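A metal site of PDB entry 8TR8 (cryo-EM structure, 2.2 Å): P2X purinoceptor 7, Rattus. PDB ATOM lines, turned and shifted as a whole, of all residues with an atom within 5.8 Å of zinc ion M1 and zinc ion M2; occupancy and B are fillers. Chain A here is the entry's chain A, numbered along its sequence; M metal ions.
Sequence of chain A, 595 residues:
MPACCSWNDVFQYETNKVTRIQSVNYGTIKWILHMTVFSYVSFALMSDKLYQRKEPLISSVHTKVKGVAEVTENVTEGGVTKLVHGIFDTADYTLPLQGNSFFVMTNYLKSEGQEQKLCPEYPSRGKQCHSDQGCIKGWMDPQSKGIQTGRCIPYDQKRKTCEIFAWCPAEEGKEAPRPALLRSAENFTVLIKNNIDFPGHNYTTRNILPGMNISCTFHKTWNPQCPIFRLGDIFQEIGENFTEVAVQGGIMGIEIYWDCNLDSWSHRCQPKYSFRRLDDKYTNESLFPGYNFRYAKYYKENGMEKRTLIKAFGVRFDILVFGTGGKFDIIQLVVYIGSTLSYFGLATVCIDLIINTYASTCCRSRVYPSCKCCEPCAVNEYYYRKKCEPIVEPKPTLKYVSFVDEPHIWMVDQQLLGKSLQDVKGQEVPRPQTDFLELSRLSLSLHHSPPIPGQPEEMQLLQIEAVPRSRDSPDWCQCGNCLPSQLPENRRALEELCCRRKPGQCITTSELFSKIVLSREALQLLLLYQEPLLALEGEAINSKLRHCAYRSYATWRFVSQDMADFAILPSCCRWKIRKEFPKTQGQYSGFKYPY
The side-chain hydroxyl (OG1) of Thr 508 sits close to the side-chain sulfur (SG) of Cys 506.
The backbone NH (N) of Gln 478 lies close to the side-chain sulfur (SG) of Cys 498 (3.3 Å).
O of Cys 479 lies close to OD1 of Asn 481 (2.6 Å).
The side-chain sulfur of Cys 482 lies close to the backbone NH of Cys 572, at 3.5 Å.
The backbone NH of Gly 480 lies close to the side-chain sulfur of Cys 477 (3.2 Å).
The backbone carbonyl oxygen (O) of Trp 476 is in hydrogen-bond range of the side-chain amide nitrogen (NE2) of Gln 478, at 2.8 Å.
Of the 17 residues printed, 4 come within 4 Å of zinc ion M1.
The nearest printed residue that does not touch zinc ion M1 is Cys 498 (4.3 Å).
Gln 478 touches zinc ion M2 (N to ZN, 3.9 Å).
Within 4 Å of zinc ion M2: Cys 477, Gln 478, Cys 479, Cys 482 and Cys 498.
The nearest printed residue that does not touch zinc ion M2 is Gly 480 (4.2 Å).
Zinc ion M1 is bound by SG of Cys 506.
Zinc ion M1 is bound by SG of Cys 499.
The side-chain sulfur (SG) of Cys 572 binds zinc ion M1 (2.3 Å).
Zinc ion M1 is bound by SG of Cys 479, at 2.3 Å.
Zinc ion M2 is bound by the side-chain sulfur of Cys 482, the side-chain sulfur of Cys 498, the side-chain sulfur of Cys 479 and the side-chain sulfur of Cys 477.
Zinc ion M2 has four donor atoms within binding distance.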
ATOM      1  N   TRP A 476      -5.030  -5.067  16.452  1.00  0.00           N
ATOM      2  CA  TRP A 476      -6.319  -5.680  16.793  1.00  0.00           C
ATOM      3  C   TRP A 476      -6.626  -5.562  18.279  1.00  0.00           C
ATOM      4  O   TRP A 476      -7.790  -5.575  18.672  1.00  0.00           O
ATOM      5  CB  TRP A 476      -6.334  -7.144  16.360  1.00  0.00           C
ATOM      6  CG  TRP A 476      -5.095  -7.900  16.663  1.00  0.00           C
ATOM      7  CD1 TRP A 476      -4.071  -8.167  15.807  1.00  0.00           C
ATOM      8  CD2 TRP A 476      -4.720  -8.493  17.909  1.00  0.00           C
ATOM      9  NE1 TRP A 476      -3.095  -8.897  16.436  1.00  0.00           N
ATOM     10  CE2 TRP A 476      -3.464  -9.108  17.732  1.00  0.00           C
ATOM     11  CE3 TRP A 476      -5.326  -8.564  19.168  1.00  0.00           C
ATOM     12  CZ2 TRP A 476      -2.815  -9.774  18.754  1.00  0.00           C
ATOM     13  CZ3 TRP A 476      -4.682  -9.235  20.184  1.00  0.00           C
ATOM     14  CH2 TRP A 476      -3.437  -9.825  19.966  1.00  0.00           C
ATOM     15  N   CYS A 477      -5.596  -5.446  19.112  1.00  0.00           N
ATOM     16  CA  CYS A 477      -5.819  -5.304  20.543  1.00  0.00           C
ATOM     17  C   CYS A 477      -6.505  -3.980  20.854  1.00  0.00           C
ATOM     18  O   CYS A 477      -6.195  -2.946  20.260  1.00  0.00           O
ATOM     19  CB  CYS A 477      -4.491  -5.393  21.309  1.00  0.00           C
ATOM     20  SG  CYS A 477      -4.637  -5.033  23.064  1.00  0.00           S
ATOM     21  N   GLN A 478      -7.439  -4.030  21.807  1.00  0.00           N
ATOM     22  CA  GLN A 478      -8.142  -2.851  22.289  1.00  0.00           C
ATOM     23  C   GLN A 478      -8.089  -2.764  23.809  1.00  0.00           C
ATOM     24  O   GLN A 478      -8.974  -2.186  24.434  1.00  0.00           O
ATOM     25  CB  GLN A 478      -9.591  -2.833  21.808  1.00  0.00           C
ATOM     26  CG  GLN A 478      -9.903  -3.631  20.549  1.00  0.00           C
ATOM     27  CD  GLN A 478      -9.646  -2.840  19.272  1.00  0.00           C
ATOM     28  OE1 GLN A 478      -9.497  -1.619  19.305  1.00  0.00           O
ATOM     29  NE2 GLN A 478      -9.600  -3.546  18.147  1.00  0.00           N
ATOM     30  N   CYS A 479      -7.052  -3.350  24.413  1.00  0.00           N
ATOM     31  CA  CYS A 479      -6.911  -3.338  25.860  1.00  0.00           C
ATOM     32  C   CYS A 479      -5.533  -2.927  26.351  1.00  0.00           C
ATOM     33  O   CYS A 479      -5.397  -2.608  27.538  1.00  0.00           O
ATOM     34  CB  CYS A 479      -7.243  -4.729  26.434  1.00  0.00           C
ATOM     35  SG  CYS A 479      -5.890  -5.932  26.451  1.00  0.00           S
ATOM     36  N   GLY A 480      -4.517  -2.908  25.491  1.00  0.00           N
ATOM     37  CA  GLY A 480      -3.208  -2.439  25.859  1.00  0.00           C
ATOM     38  C   GLY A 480      -2.342  -3.453  26.585  1.00  0.00           C
ATOM     39  O   GLY A 480      -1.197  -3.120  26.935  1.00  0.00           O
ATOM     40  N   ASN A 481      -2.840  -4.662  26.823  1.00  0.00           N
ATOM     41  CA  ASN A 481      -2.087  -5.681  27.539  1.00  0.00           C
ATOM     42  C   ASN A 481      -1.762  -6.898  26.689  1.00  0.00           C
ATOM     43  O   ASN A 481      -0.954  -7.733  27.129  1.00  0.00           O
ATOM     44  CB  ASN A 481      -2.871  -6.141  28.777  1.00  0.00           C
ATOM     45  CG  ASN A 481      -3.439  -4.983  29.570  1.00  0.00           C
ATOM     46  OD1 ASN A 481      -4.443  -4.393  29.190  1.00  0.00           O
ATOM     47  ND2 ASN A 481      -2.787  -4.662  30.683  1.00  0.00           N
ATOM     48  N   CYS A 482      -2.336  -7.022  25.495  1.00  0.00           N
ATOM     49  CA  CYS A 482      -2.045  -8.161  24.641  1.00  0.00           C
ATOM     50  C   CYS A 482      -0.649  -8.052  24.050  1.00  0.00           C
ATOM     51  O   CYS A 482      -0.072  -6.960  23.928  1.00  0.00           O
ATOM     52  CB  CYS A 482      -3.083  -8.250  23.525  1.00  0.00           C
ATOM     53  SG  CYS A 482      -4.744  -8.688  24.074  1.00  0.00           S
ATOM     54  N   LEU A 497      -6.038 -12.538  19.460  1.00  0.00           N
ATOM     55  CA  LEU A 497      -7.361 -12.299  20.025  1.00  0.00           C
ATOM     56  C   LEU A 497      -7.237 -11.419  21.253  1.00  0.00           C
ATOM     57  O   LEU A 497      -6.309 -11.582  22.053  1.00  0.00           O
ATOM     58  CB  LEU A 497      -8.036 -13.619  20.370  1.00  0.00           C
ATOM     59  CG  LEU A 497      -9.450 -13.612  20.948  1.00  0.00           C
ATOM     60  CD1 LEU A 497     -10.461 -13.162  19.919  1.00  0.00           C
ATOM     61  CD2 LEU A 497      -9.774 -14.986  21.471  1.00  0.00           C
ATOM     62  N   CYS A 498      -8.175 -10.486  21.394  1.00  0.00           N
ATOM     63  CA  CYS A 498      -8.217  -9.578  22.524  1.00  0.00           C
ATOM     64  C   CYS A 498      -9.475  -9.835  23.344  1.00  0.00           C
ATOM     65  O   CYS A 498     -10.449 -10.417  22.868  1.00  0.00           O
ATOM     66  CB  CYS A 498      -8.169  -8.105  22.071  1.00  0.00           C
ATOM     67  SG  CYS A 498      -8.013  -6.896  23.409  1.00  0.00           S
ATOM     68  N   CYS A 499      -9.426  -9.391  24.608  1.00  0.00           N
ATOM     69  CA  CYS A 499     -10.557  -9.536  25.508  1.00  0.00           C
ATOM     70  C   CYS A 499     -11.783  -8.751  25.068  1.00  0.00           C
ATOM     71  O   CYS A 499     -12.872  -9.014  25.592  1.00  0.00           O
ATOM     72  CB  CYS A 499     -10.149  -9.089  26.915  1.00  0.00           C
ATOM     73  SG  CYS A 499      -9.334  -7.485  26.987  1.00  0.00           S
ATOM     74  N   ARG A 500     -11.641  -7.799  24.147  1.00  0.00           N
ATOM     75  CA  ARG A 500     -12.751  -6.930  23.787  1.00  0.00           C
ATOM     76  C   ARG A 500     -12.614  -6.514  22.326  1.00  0.00           C
ATOM     77  O   ARG A 500     -11.533  -6.586  21.737  1.00  0.00           O
ATOM     78  CB  ARG A 500     -12.802  -5.706  24.682  1.00  0.00           C
ATOM     79  CG  ARG A 500     -11.494  -4.958  24.776  1.00  0.00           C
ATOM     80  CD  ARG A 500     -11.509  -3.931  25.883  1.00  0.00           C
ATOM     81  NE  ARG A 500     -12.845  -3.398  26.114  1.00  0.00           N
ATOM     82  CZ  ARG A 500     -13.369  -3.159  27.307  1.00  0.00           C
ATOM     83  NH1 ARG A 500     -12.690  -3.415  28.410  1.00  0.00           N
ATOM     84  NH2 ARG A 500     -14.598  -2.674  27.398  1.00  0.00           N
ATOM     85  N   CYS A 506      -8.900  -3.753  30.350  1.00  0.00           N
ATOM     86  CA  CYS A 506      -8.723  -5.189  30.174  1.00  0.00           C
ATOM     87  C   CYS A 506      -9.456  -5.958  31.265  1.00  0.00           C
ATOM     88  O   CYS A 506      -9.587  -5.502  32.410  1.00  0.00           O
ATOM     89  CB  CYS A 506      -7.236  -5.545  30.181  1.00  0.00           C
ATOM     90  SG  CYS A 506      -6.887  -7.284  29.861  1.00  0.00           S
ATOM     91  N   ILE A 507      -9.934  -7.154  30.908  1.00  0.00           N
ATOM     92  CA  ILE A 507     -10.617  -8.017  31.866  1.00  0.00           C
ATOM     93  C   ILE A 507      -9.680  -8.408  32.998  1.00  0.00           C
ATOM     94  O   ILE A 507     -10.130  -8.694  34.118  1.00  0.00           O
ATOM     95  CB  ILE A 507     -11.180  -9.253  31.144  1.00  0.00           C
ATOM     96  CG1 ILE A 507     -12.019 -10.093  32.120  1.00  0.00           C
ATOM     97  CG2 ILE A 507     -10.061 -10.089  30.559  1.00  0.00           C
ATOM     98  CD1 ILE A 507     -12.916 -11.092  31.440  1.00  0.00           C
ATOM     99  N   THR A 508      -8.369  -8.437  32.745  1.00  0.00           N
ATOM    100  CA  THR A 508      -7.412  -8.801  33.781  1.00  0.00           C
ATOM    101  C   THR A 508      -7.444  -7.864  34.970  1.00  0.00           C
ATOM    102  O   THR A 508      -7.026  -8.247  36.066  1.00  0.00           O
ATOM    103  CB  THR A 508      -5.995  -8.830  33.203  1.00  0.00           C
ATOM    104  OG1 THR A 508      -5.680  -7.543  32.649  1.00  0.00           O
ATOM    105  CG2 THR A 508      -5.885  -9.879  32.112  1.00  0.00           C
ATOM    106  N   PRO A 570      -8.002 -14.931  25.254  1.00  0.00           N
ATOM    107  CA  PRO A 570      -7.341 -13.715  24.761  1.00  0.00           C
ATOM    108  C   PRO A 570      -5.864 -13.723  25.075  1.00  0.00           C
ATOM    109  O   PRO A 570      -5.383 -14.370  26.009  1.00  0.00           O
ATOM    110  CB  PRO A 570      -8.071 -12.590  25.500  1.00  0.00           C
ATOM    111  CG  PRO A 570      -9.323 -13.188  25.978  1.00  0.00           C
ATOM    112  CD  PRO A 570      -9.041 -14.616  26.235  1.00  0.00           C
ATOM    113  N   CYS A 572      -3.957 -11.299  26.227  1.00  0.00           N
ATOM    114  CA  CYS A 572      -3.628 -10.683  27.508  1.00  0.00           C
ATOM    115  C   CYS A 572      -3.734 -11.675  28.654  1.00  0.00           C
ATOM    116  O   CYS A 572      -2.798 -11.837  29.448  1.00  0.00           O
ATOM    117  CB  CYS A 572      -4.545  -9.480  27.739  1.00  0.00           C
ATOM    118  SG  CYS A 572      -6.220  -9.718  27.129  1.00  0.00           S
ATOM    119  N   CYS A 573      -4.888 -12.342  28.763  1.00  0.00           N
ATOM    120  CA  CYS A 573      -5.094 -13.313  29.839  1.00  0.00           C
ATOM    121  C   CYS A 573      -4.115 -14.467  29.715  1.00  0.00           C
ATOM    122  O   CYS A 573      -3.544 -14.934  30.707  1.00  0.00           O
ATOM    123  CB  CYS A 573      -6.536 -13.807  29.792  1.00  0.00           C
ATOM    124  SG  CYS A 573      -7.728 -12.485  29.509  1.00  0.00           S
HETATM  125 ZN    ZN M   1      -7.083  -7.598  27.568  1.00  0.00          ZN
HETATM  126 ZN    ZN M   2      -5.852  -6.650  24.236  1.00  0.00          ZN
